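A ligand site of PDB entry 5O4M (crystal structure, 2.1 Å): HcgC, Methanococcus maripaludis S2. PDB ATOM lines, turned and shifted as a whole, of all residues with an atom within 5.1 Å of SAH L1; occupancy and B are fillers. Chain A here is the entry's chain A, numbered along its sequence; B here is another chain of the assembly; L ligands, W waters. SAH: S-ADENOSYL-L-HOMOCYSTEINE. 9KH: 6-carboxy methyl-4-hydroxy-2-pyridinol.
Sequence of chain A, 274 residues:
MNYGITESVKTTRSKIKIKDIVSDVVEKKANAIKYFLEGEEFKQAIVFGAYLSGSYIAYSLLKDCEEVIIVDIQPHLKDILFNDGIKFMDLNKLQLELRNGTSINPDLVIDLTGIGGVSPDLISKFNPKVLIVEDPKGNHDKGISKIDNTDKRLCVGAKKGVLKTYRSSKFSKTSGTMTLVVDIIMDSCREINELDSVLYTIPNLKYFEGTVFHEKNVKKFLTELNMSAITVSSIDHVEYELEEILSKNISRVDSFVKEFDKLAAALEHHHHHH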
ATOM      1  N   LYS A  29      -2.802   3.755 -15.949  1.00  0.00           N
ATOM      2  CA  LYS A  29      -3.006   2.659 -14.999  1.00  0.00           C
ATOM      3  C   LYS A  29      -3.296   3.219 -13.625  1.00  0.00           C
ATOM      4  O   LYS A  29      -4.235   2.771 -12.949  1.00  0.00           O
ATOM      5  CB  LYS A  29      -1.803   1.689 -14.996  1.00  0.00           C
ATOM      6  CG  LYS A  29      -1.641   0.904 -16.293  1.00  0.00           C
ATOM      7  CD  LYS A  29      -0.481  -0.063 -16.229  1.00  0.00           C
ATOM      8  CE  LYS A  29      -0.395  -0.964 -17.449  1.00  0.00           C
ATOM      9  NZ  LYS A  29       0.578  -2.046 -17.302  1.00  0.00           N
ATOM     10  N   PHE A  48       2.509  -4.971  -4.869  1.00  0.00           N
ATOM     11  CA  PHE A  48       3.481  -5.979  -5.276  1.00  0.00           C
ATOM     12  C   PHE A  48       3.892  -5.746  -6.714  1.00  0.00           C
ATOM     13  O   PHE A  48       3.045  -5.754  -7.600  1.00  0.00           O
ATOM     14  CB  PHE A  48       2.899  -7.400  -5.134  1.00  0.00           C
ATOM     15  CG  PHE A  48       2.701  -7.839  -3.708  1.00  0.00           C
ATOM     16  CD1 PHE A  48       1.522  -7.561  -3.032  1.00  0.00           C
ATOM     17  CD2 PHE A  48       3.684  -8.555  -3.040  1.00  0.00           C
ATOM     18  CE1 PHE A  48       1.333  -7.986  -1.707  1.00  0.00           C
ATOM     19  CE2 PHE A  48       3.505  -8.974  -1.723  1.00  0.00           C
ATOM     20  CZ  PHE A  48       2.331  -8.696  -1.066  1.00  0.00           C
ATOM     21  N   GLY A  49       5.204  -5.539  -6.925  1.00  0.00           N
ATOM     22  CA  GLY A  49       5.783  -5.325  -8.243  1.00  0.00           C
ATOM     23  C   GLY A  49       6.153  -3.897  -8.504  1.00  0.00           C
ATOM     24  O   GLY A  49       5.298  -3.127  -8.919  1.00  0.00           O
ATOM     25  N   ALA A  50       7.430  -3.526  -8.284  1.00  0.00           N
ATOM     26  CA  ALA A  50       7.893  -2.161  -8.524  1.00  0.00           C
ATOM     27  C   ALA A  50       7.995  -1.856 -10.021  1.00  0.00           C
ATOM     28  O   ALA A  50       7.626  -0.744 -10.454  1.00  0.00           O
ATOM     29  CB  ALA A  50       9.242  -1.917  -7.857  1.00  0.00           C
ATOM     30  N   TYR A  51       8.491  -2.802 -10.812  1.00  0.00           N
ATOM     31  CA  TYR A  51       8.593  -2.526 -12.247  1.00  0.00           C
ATOM     32  C   TYR A  51       7.316  -2.973 -12.979  1.00  0.00           C
ATOM     33  O   TYR A  51       6.800  -3.994 -12.652  1.00  0.00           O
ATOM     34  CB  TYR A  51       9.831  -3.177 -12.793  1.00  0.00           C
ATOM     35  CG  TYR A  51       9.955  -3.370 -14.280  1.00  0.00           C
ATOM     36  CD1 TYR A  51       9.287  -4.398 -14.930  1.00  0.00           C
ATOM     37  CD2 TYR A  51      10.812  -2.569 -15.030  1.00  0.00           C
ATOM     38  CE1 TYR A  51       9.435  -4.601 -16.299  1.00  0.00           C
ATOM     39  CE2 TYR A  51      10.993  -2.781 -16.391  1.00  0.00           C
ATOM     40  CZ  TYR A  51      10.294  -3.793 -17.028  1.00  0.00           C
ATOM     41  OH  TYR A  51      10.473  -3.977 -18.369  1.00  0.00           O
ATOM     42  N   LEU A  52       6.869  -2.285 -14.008  1.00  0.00           N
ATOM     43  CA  LEU A  52       7.383  -0.993 -14.502  1.00  0.00           C
ATOM     44  C   LEU A  52       6.427   0.099 -14.011  1.00  0.00           C
ATOM     45  O   LEU A  52       6.858   1.180 -13.680  1.00  0.00           O
ATOM     46  CB  LEU A  52       7.454  -0.977 -16.044  1.00  0.00           C
ATOM     47  CG  LEU A  52       7.942   0.339 -16.708  1.00  0.00           C
ATOM     48  CD1 LEU A  52       9.216   0.857 -16.070  1.00  0.00           C
ATOM     49  CD2 LEU A  52       8.206   0.143 -18.204  1.00  0.00           C
ATOM     50  N   SER A  53       5.166  -0.189 -13.951  1.00  0.00           N
ATOM     51  CA  SER A  53       4.105   0.747 -13.522  1.00  0.00           C
ATOM     52  C   SER A  53       3.929   0.881 -11.985  1.00  0.00           C
ATOM     53  O   SER A  53       3.324   1.856 -11.506  1.00  0.00           O
ATOM     54  CB  SER A  53       2.806   0.380 -14.228  1.00  0.00           C
ATOM     55  OG  SER A  53       2.421  -0.969 -13.972  1.00  0.00           O
ATOM     56  N   VAL A  71       6.431  -3.794  -2.551  1.00  0.00           N
ATOM     57  CA  VAL A  71       7.091  -5.067  -2.236  1.00  0.00           C
ATOM     58  C   VAL A  71       7.604  -5.671  -3.580  1.00  0.00           C
ATOM     59  O   VAL A  71       6.881  -5.687  -4.571  1.00  0.00           O
ATOM     60  CB  VAL A  71       6.166  -6.062  -1.499  1.00  0.00           C
ATOM     61  CG1 VAL A  71       6.908  -7.377  -1.206  1.00  0.00           C
ATOM     62  CG2 VAL A  71       5.622  -5.456  -0.213  1.00  0.00           C
ATOM     63  N   ASP A  72       8.851  -6.155  -3.593  1.00  0.00           N
ATOM     64  CA  ASP A  72       9.396  -6.783  -4.796  1.00  0.00           C
ATOM     65  C   ASP A  72      10.308  -7.897  -4.416  1.00  0.00           C
ATOM     66  O   ASP A  72      11.033  -7.824  -3.415  1.00  0.00           O
ATOM     67  CB  ASP A  72      10.120  -5.808  -5.773  1.00  0.00           C
ATOM     68  CG  ASP A  72      10.100  -6.289  -7.227  1.00  0.00           C
ATOM     69  OD1 ASP A  72      10.839  -7.240  -7.553  1.00  0.00           O
ATOM     70  OD2 ASP A  72       9.318  -5.721  -8.033  1.00  0.00           O
ATOM     71  N   ILE A  73      10.305  -8.935  -5.215  1.00  0.00           N
ATOM     72  CA  ILE A  73      11.170 -10.081  -4.999  1.00  0.00           C
ATOM     73  C   ILE A  73      12.654  -9.672  -5.266  1.00  0.00           C
ATOM     74  O   ILE A  73      13.573 -10.299  -4.736  1.00  0.00           O
ATOM     75  CB  ILE A  73      10.664 -11.311  -5.815  1.00  0.00           C
ATOM     76  CG1 ILE A  73      11.336 -12.614  -5.302  1.00  0.00           C
ATOM     77  CG2 ILE A  73      10.863 -11.141  -7.330  1.00  0.00           C
ATOM     78  CD1 ILE A  73      10.606 -13.929  -5.799  1.00  0.00           C
ATOM     79  N   GLN A  74      12.882  -8.607  -6.077  1.00  0.00           N
ATOM     80  CA  GLN A  74      14.208  -8.096  -6.422  1.00  0.00           C
ATOM     81  C   GLN A  74      14.582  -6.942  -5.491  1.00  0.00           C
ATOM     82  O   GLN A  74      14.047  -5.841  -5.674  1.00  0.00           O
ATOM     83  CB  GLN A  74      14.216  -7.572  -7.881  1.00  0.00           C
ATOM     84  CG  GLN A  74      13.866  -8.599  -8.942  1.00  0.00           C
ATOM     85  CD  GLN A  74      14.919  -9.657  -9.146  1.00  0.00           C
ATOM     86  OE1 GLN A  74      16.119  -9.436  -8.952  1.00  0.00           O
ATOM     87  NE2 GLN A  74      14.505 -10.817  -9.605  1.00  0.00           N
ATOM     88  N   LEU A  77      15.352  -3.268  -6.896  1.00  0.00           N
ATOM     89  CA  LEU A  77      14.293  -2.433  -7.450  1.00  0.00           C
ATOM     90  C   LEU A  77      13.911  -1.263  -6.544  1.00  0.00           C
ATOM     91  O   LEU A  77      13.094  -0.445  -6.951  1.00  0.00           O
ATOM     92  CB  LEU A  77      13.080  -3.240  -7.927  1.00  0.00           C
ATOM     93  CG  LEU A  77      13.274  -3.885  -9.321  1.00  0.00           C
ATOM     94  CD1 LEU A  77      12.136  -4.776  -9.678  1.00  0.00           C
ATOM     95  CD2 LEU A  77      13.404  -2.826 -10.411  1.00  0.00           C
ATOM     96  N   LEU A  91      10.606  -9.231  -0.820  1.00  0.00           N
ATOM     97  CA  LEU A  91       9.673 -10.308  -0.463  1.00  0.00           C
ATOM     98  C   LEU A  91      10.051 -11.070   0.818  1.00  0.00           C
ATOM     99  O   LEU A  91       9.149 -11.429   1.584  1.00  0.00           O
ATOM    100  CB  LEU A  91       9.504 -11.284  -1.638  1.00  0.00           C
ATOM    101  CG  LEU A  91       8.362 -12.268  -1.585  1.00  0.00           C
ATOM    102  CD1 LEU A  91       7.024 -11.573  -1.522  1.00  0.00           C
ATOM    103  CD2 LEU A  91       8.407 -13.173  -2.784  1.00  0.00           C
ATOM    104  N   LEU A 112       0.555  -6.178  -8.971  1.00  0.00           N
ATOM    105  CA  LEU A 112       0.957  -5.760 -10.310  1.00  0.00           C
ATOM    106  C   LEU A 112       2.026  -6.697 -10.901  1.00  0.00           C
ATOM    107  O   LEU A 112       2.561  -6.403 -11.964  1.00  0.00           O
ATOM    108  CB  LEU A 112       1.546  -4.348 -10.256  1.00  0.00           C
ATOM    109  CG  LEU A 112       0.684  -3.249  -9.662  1.00  0.00           C
ATOM    110  CD1 LEU A 112       1.455  -1.985  -9.596  1.00  0.00           C
ATOM    111  CD2 LEU A 112      -0.581  -3.044 -10.438  1.00  0.00           C
ATOM    112  N   THR A 113       2.338  -7.813 -10.246  1.00  0.00           N
ATOM    113  CA  THR A 113       3.364  -8.747 -10.713  1.00  0.00           C
ATOM    114  C   THR A 113       3.024  -9.526 -12.030  1.00  0.00           C
ATOM    115  O   THR A 113       3.940  -9.884 -12.795  1.00  0.00           O
ATOM    116  CB  THR A 113       3.744  -9.693  -9.562  1.00  0.00           C
ATOM    117  OG1 THR A 113       2.661 -10.576  -9.251  1.00  0.00           O
ATOM    118  CG2 THR A 113       4.195  -8.929  -8.322  1.00  0.00           C
ATOM    119  N   GLY A 114       1.748  -9.769 -12.282  1.00  0.00           N
ATOM    120  CA  GLY A 114       1.346 -10.494 -13.470  1.00  0.00           C
ATOM    121  C   GLY A 114       1.905 -11.893 -13.617  1.00  0.00           C
ATOM    122  O   GLY A 114       1.922 -12.664 -12.641  1.00  0.00           O
ATOM    123  N   GLY A 116       3.794 -15.242 -13.701  1.00  0.00           N
ATOM    124  CA  GLY A 116       4.748 -15.887 -12.814  1.00  0.00           C
ATOM    125  C   GLY A 116       5.061 -15.142 -11.544  1.00  0.00           C
ATOM    126  O   GLY A 116       6.063 -15.448 -10.896  1.00  0.00           O
ATOM    127  N   GLY A 117       4.204 -14.190 -11.182  1.00  0.00           N
ATOM    128  CA  GLY A 117       4.329 -13.347 -10.016  1.00  0.00           C
ATOM    129  C   GLY A 117       3.848 -13.929  -8.703  1.00  0.00           C
ATOM    130  O   GLY A 117       3.942 -15.127  -8.463  1.00  0.00           O
ATOM    131  N   VAL A 118       3.324 -13.045  -7.836  1.00  0.00           N
ATOM    132  CA  VAL A 118       2.828 -13.421  -6.487  1.00  0.00           C
ATOM    133  C   VAL A 118       1.876 -14.567  -6.523  1.00  0.00           C
ATOM    134  O   VAL A 118       1.032 -14.688  -7.397  1.00  0.00           O
ATOM    135  CB  VAL A 118       2.216 -12.305  -5.611  1.00  0.00           C
ATOM    136  CG1 VAL A 118       3.152 -11.144  -5.436  1.00  0.00           C
ATOM    137  CG2 VAL A 118       0.868 -11.840  -6.123  1.00  0.00           C
ATOM    138  N   SER A 119       2.007 -15.395  -5.521  1.00  0.00           N
ATOM    139  CA  SER A 119       1.200 -16.580  -5.371  1.00  0.00           C
ATOM    140  C   SER A 119      -0.121 -16.271  -4.727  1.00  0.00           C
ATOM    141  O   SER A 119      -0.148 -15.458  -3.799  1.00  0.00           O
ATOM    142  CB  SER A 119       1.939 -17.578  -4.477  1.00  0.00           C
ATOM    143  OG  SER A 119       2.117 -17.058  -3.162  1.00  0.00           O
ATOM    144  N   GLU A 134      -3.682  -6.901 -11.201  1.00  0.00           N
ATOM    145  CA  GLU A 134      -3.495  -6.504 -12.588  1.00  0.00           C
ATOM    146  C   GLU A 134      -3.563  -7.736 -13.481  1.00  0.00           C
ATOM    147  O   GLU A 134      -2.831  -8.688 -13.256  1.00  0.00           O
ATOM    148  CB  GLU A 134      -2.133  -5.832 -12.814  1.00  0.00           C
ATOM    149  CG  GLU A 134      -1.909  -5.444 -14.274  1.00  0.00           C
ATOM    150  CD  GLU A 134      -0.923  -4.342 -14.538  1.00  0.00           C
ATOM    151  OE1 GLU A 134       0.044  -4.200 -13.749  1.00  0.00           O
ATOM    152  OE2 GLU A 134      -1.069  -3.668 -15.582  1.00  0.00           O
ATOM    153  N   SER A 175      -0.835  -6.665 -21.265  1.00  0.00           N
ATOM    154  CA  SER A 175      -1.223  -5.400 -20.721  1.00  0.00           C
ATOM    155  C   SER A 175      -0.014  -4.749 -20.079  1.00  0.00           C
ATOM    156  O   SER A 175      -0.152  -3.651 -19.507  1.00  0.00           O
ATOM    157  CB  SER A 175      -2.288  -5.600 -19.665  1.00  0.00           C
ATOM    158  OG  SER A 175      -1.764  -6.406 -18.627  1.00  0.00           O
ATOM    159  N   GLY A 176       1.146  -5.390 -20.171  1.00  0.00           N
ATOM    160  CA  GLY A 176       2.334  -4.830 -19.563  1.00  0.00           C
ATOM    161  C   GLY A 176       2.777  -3.518 -20.186  1.00  0.00           C
ATOM    162  O   GLY A 176       2.713  -3.353 -21.401  1.00  0.00           O
ATOM    163  N   THR A 177       3.223  -2.575 -19.349  1.00  0.00           N
ATOM    164  CA  THR A 177       3.720  -1.268 -19.765  1.00  0.00           C
ATOM    165  C   THR A 177       4.796  -1.438 -20.793  1.00  0.00           C
ATOM    166  O   THR A 177       4.750  -0.707 -21.785  1.00  0.00           O
ATOM    167  CB  THR A 177       4.267  -0.553 -18.575  1.00  0.00           C
ATOM    168  OG1 THR A 177       3.259  -0.685 -17.620  1.00  0.00           O
ATOM    169  CG2 THR A 177       4.617   0.920 -18.861  1.00  0.00           C
ATOM    170  N   MET A 178       5.744  -2.397 -20.591  1.00  0.00           N
ATOM    171  CA  MET A 178       6.820  -2.603 -21.599  1.00  0.00           C
ATOM    172  C   MET A 178       6.275  -3.034 -22.966  1.00  0.00           C
ATOM    173  O   MET A 178       6.659  -2.496 -24.023  1.00  0.00           O
ATOM    174  CB  MET A 178       7.864  -3.599 -21.129  1.00  0.00           C
ATOM    175  CG  MET A 178       8.982  -3.828 -22.168  1.00  0.00           C
ATOM    176  SD  MET A 178      10.012  -2.345 -22.569  1.00  0.00           S
ATOM    177  CE  MET A 178      10.490  -1.847 -20.982  1.00  0.00           C
ATOM    178  N   PHE A 213      16.623  -6.355 -14.960  1.00  0.00           N
ATOM    179  CA  PHE A 213      16.676  -7.658 -14.278  1.00  0.00           C
ATOM    180  C   PHE A 213      17.908  -8.565 -14.485  1.00  0.00           C
ATOM    181  O   PHE A 213      18.101  -9.518 -13.703  1.00  0.00           O
ATOM    182  CB  PHE A 213      15.425  -8.456 -14.682  1.00  0.00           C
ATOM    183  CG  PHE A 213      14.198  -7.713 -14.257  1.00  0.00           C
ATOM    184  CD1 PHE A 213      13.667  -7.880 -12.981  1.00  0.00           C
ATOM    185  CD2 PHE A 213      13.580  -6.801 -15.102  1.00  0.00           C
ATOM    186  CE1 PHE A 213      12.570  -7.161 -12.557  1.00  0.00           C
ATOM    187  CE2 PHE A 213      12.478  -6.075 -14.691  1.00  0.00           C
ATOM    188  CZ  PHE A 213      11.968  -6.250 -13.409  1.00  0.00           C
ATOM    189  N   ILE B   5      11.930 -11.820 -16.419  1.00  0.00           N
ATOM    190  CA  ILE B   5      11.697 -11.221 -15.095  1.00  0.00           C
ATOM    191  C   ILE B   5      11.608 -12.354 -14.016  1.00  0.00           C
ATOM    192  O   ILE B   5      12.016 -12.167 -12.892  1.00  0.00           O
ATOM    193  CB  ILE B   5      10.401 -10.344 -15.159  1.00  0.00           C
ATOM    194  CG1 ILE B   5      10.633  -9.158 -16.114  1.00  0.00           C
ATOM    195  CG2 ILE B   5       9.992  -9.868 -13.769  1.00  0.00           C
ATOM    196  CD1 ILE B   5       9.436  -8.350 -16.544  1.00  0.00           C
ATOM    197  N   THR B   6      11.045 -13.504 -14.395  1.00  0.00           N
ATOM    198  CA  THR B   6      10.886 -14.687 -13.536  1.00  0.00           C
ATOM    199  C   THR B   6      11.169 -15.887 -14.433  1.00  0.00           C
ATOM    200  O   THR B   6      11.339 -15.723 -15.658  1.00  0.00           O
ATOM    201  CB  THR B   6       9.418 -14.822 -12.961  1.00  0.00           C
ATOM    202  OG1 THR B   6       8.519 -15.144 -14.009  1.00  0.00           O
ATOM    203  CG2 THR B   6       8.950 -13.616 -12.177  1.00  0.00           C
HETATM  204  N   SAH L   1       2.544  -5.307 -14.429  1.00  0.00           N
HETATM  205  CA  SAH L   1       3.840  -4.609 -14.577  1.00  0.00           C
HETATM  206  CB  SAH L   1       4.919  -5.625 -15.011  1.00  0.00           C
HETATM  207  CG  SAH L   1       5.252  -6.603 -13.891  1.00  0.00           C
HETATM  208  SD  SAH L   1       6.799  -7.419 -14.049  1.00  0.00           S
HETATM  209  C   SAH L   1       3.702  -3.574 -15.644  1.00  0.00           C
HETATM  210  O   SAH L   1       4.569  -2.706 -15.706  1.00  0.00           O
HETATM  211  OXT SAH L   1       2.737  -3.596 -16.434  1.00  0.00           O
HETATM  212  C5' SAH L   1       6.932  -8.300 -12.523  1.00  0.00           C
HETATM  213  C4' SAH L   1       7.443  -7.362 -11.395  1.00  0.00           C
HETATM  214  O4' SAH L   1       7.057  -7.901 -10.133  1.00  0.00           O
HETATM  215  C3' SAH L   1       8.967  -7.348 -11.352  1.00  0.00           C
HETATM  216  O3' SAH L   1       9.468  -6.131 -10.710  1.00  0.00           O
HETATM  217  C2' SAH L   1       9.297  -8.586 -10.526  1.00  0.00           C
HETATM  218  O2' SAH L   1      10.612  -8.532  -9.926  1.00  0.00           O
HETATM  219  C1' SAH L   1       8.209  -8.501  -9.469  1.00  0.00           C
HETATM  220  N9  SAH L   1       7.793  -9.807  -8.933  1.00  0.00           N
HETATM  221  C8  SAH L   1       7.665 -10.979  -9.604  1.00  0.00           C
HETATM  222  N7  SAH L   1       7.222 -11.937  -8.739  1.00  0.00           N
HETATM  223  C5  SAH L   1       7.037 -11.356  -7.506  1.00  0.00           C
HETATM  224  C6  SAH L   1       6.571 -11.769  -6.140  1.00  0.00           C
HETATM  225  N6  SAH L   1       6.194 -13.041  -5.862  1.00  0.00           N
HETATM  226  N1  SAH L   1       6.539 -10.842  -5.154  1.00  0.00           N
HETATM  227  C2  SAH L   1       6.913  -9.563  -5.382  1.00  0.00           C
HETATM  228  N3  SAH L   1       7.339  -9.127  -6.593  1.00  0.00           N
HETATM  229  C4  SAH L   1       7.405  -9.949  -7.665  1.00  0.00           C
HETATM  230  C2  9KH L   2       4.223  -9.496 -16.753  1.00  0.00           C
HETATM  231  C3  9KH L   2       4.187  -8.815 -17.968  1.00  0.00           C
HETATM  232  C4  9KH L   2       5.269  -8.978 -18.861  1.00  0.00           C
HETATM  233  C6  9KH L   2       6.330 -10.477 -17.327  1.00  0.00           C
HETATM  234  O1  9KH L   2       3.175  -9.328 -15.913  1.00  0.00           O
HETATM  235  N5  9KH L   2       6.296  -9.788 -18.510  1.00  0.00           N
HETATM  236  C7  9KH L   2       5.293 -10.337 -16.413  1.00  0.00           C
HETATM  237  O8  9KH L   2       7.403 -11.275 -17.048  1.00  0.00           O
HETATM  238  C9  9KH L   2       2.962  -7.942 -18.220  1.00  0.00           C
HETATM  239  C10 9KH L   2       5.393  -8.265 -20.194  1.00  0.00           C
HETATM  240  C12 9KH L   2       5.720  -6.793 -19.923  1.00  0.00           C
HETATM  241  O13 9KH L   2       6.413  -6.442 -18.921  1.00  0.00           O
HETATM  242  O14 9KH L   2       5.262  -5.936 -20.721  1.00  0.00           O
HETATM  243  O   HOH W   1       0.717  -7.786 -14.963  1.00  0.00           O
HETATM  244  O   HOH W   2       7.508 -14.878  -8.674  1.00  0.00           O
HETATM  245  O   HOH W   3       4.968 -15.324  -4.123  1.00  0.00           O
HETATM  246  O   HOH W   4      11.801 -10.837 -10.639  1.00  0.00           O
HETATM  247  O   HOH W   5       6.285  -3.843 -17.985  1.00  0.00           O
HETATM  248  O   HOH W   6       6.005 -11.589 -12.305  1.00  0.00           O
HETATM  249  O   HOH W   7       0.340  -6.036 -16.880  1.00  0.00           O
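N of Ile 73 is in hydrogen-bond range of N3 of SAH L1 (3.3 Å).
N of SAH L1 lies within hydrogen-bond range of O of Leu 112.
OG1 of Thr 177 sits at hydrogen-bond distance from O of SAH L1 (3.1 Å).
O of SAH L1 sits at hydrogen-bond distance from N of Ser 53.
OE1 of Glu 134 lies within salt-bridge range of N of SAH L1 (2.8 Å).
OXT of SAH L1 is in hydrogen-bond range of N of Thr 177 (3.1 Å).
The side-chain hydroxyl (OG) of Ser 53 sits at hydrogen-bond distance from an oxygen (O) of SAH L1 (3.3 Å).
N of Leu 52 is in hydrogen-bond range of O of SAH L1 (2.9 Å).
NZ of Lys 29 is in salt-bridge range of OXT of SAH L1 (2.8 Å).
O of Thr 113 is in hydrogen-bond range of O1 of 9KH L2, at 3.3 Å.
An oxygen (O3') of SAH L1 is in hydrogen-bond range of the backbone NH (N) of Tyr 51.
The side-chain carboxylate (OD1) of Asp 72 sits at hydrogen-bond distance from an oxygen (O2') of SAH L1 (2.7 Å).
Water W4 lies within hydrogen-bond range of O of Ile 5 of chain B (2.6 Å), O2' of SAH L1 (2.7 Å) and NE2 of Gln 74 (2.9 Å).
Water W2 lies within hydrogen-bond range of the backbone carbonyl oxygen of Gly 116 and a nitrogen (N7) of SAH L1.
Water W5 lies within hydrogen-bond range of O13 of 9KH L2 (2.8 Å), N of Met 178 (3.0 Å) and O of SAH L1 (3.1 Å).
Water W3 bridges a nitrogen (N6) of SAH L1 (3.1 Å) and the backbone NH of Ser 119 (3.3 Å).
Water W1 lies within hydrogen-bond range of O1 of 9KH L2 (3.1 Å), N of SAH L1 (3.1 Å) and N of Gly 114 (3.5 Å).
Water W7 lies within hydrogen-bond range of OG of Ser 175 (2.8 Å), OE2 of Glu 134 (3.0 Å), N of SAH L1 (3.4 Å) and N of Gly 176 (3.4 Å).
The backbone NH of Thr 113 lies within hydrogen-bond range of the backbone carbonyl oxygen of Phe 48 (3.4 Å).
The side-chain amino group (NZ) of Lys 29 lies within salt-bridge range of the side-chain carboxylate (OE2) of Glu 134 (2.9 Å).
N of Leu 112 is in hydrogen-bond range of O of Phe 48 (2.9 Å).
OG1 of Thr 177 lies within hydrogen-bond range of NZ of Lys 29 (3.0 Å).
The backbone NH (N) of Ala 50 sits at hydrogen-bond distance from the side-chain carboxylate (OD2) of Asp 72 (2.9 Å).
The backbone NH (N) of Leu 91 lies within hydrogen-bond range of the backbone carbonyl oxygen (O) of Asp 72 (3.0 Å).
The backbone carbonyl oxygen of Val 71 lies within hydrogen-bond range of the backbone NH of Gly 49 (2.9 Å).
The side-chain carboxylate (OD1) of Asp 72 lies within hydrogen-bond range of the backbone NH (N) of Gln 74.
The backbone NH (N) of Val 118 lies close to a nitrogen (N6) of SAH L1.
Merely in contact with SAH L1: Leu 77, Gly 176, Thr 113, Gln 74, Gly 49, Gly 117, Phe 213, Ile 5 of chain B, Leu 91, Thr 6 of chain B and Val 71.
Within 4 Å of SAH L1: Lys 29, Gly 49, Tyr 51, Leu 52, Ser 53, Val 71, Asp 72, Ile 73, Gln 74, Leu 77, Leu 91, Leu 112, Thr 113, Gly 117, Val 118, Glu 134, Gly 176, Thr 177, Phe 213, Ile 5 of chain B and Thr 6 of chain B.
The nearest printed residue that does not touch SAH L1 is Ala 50 (4.1 Å).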
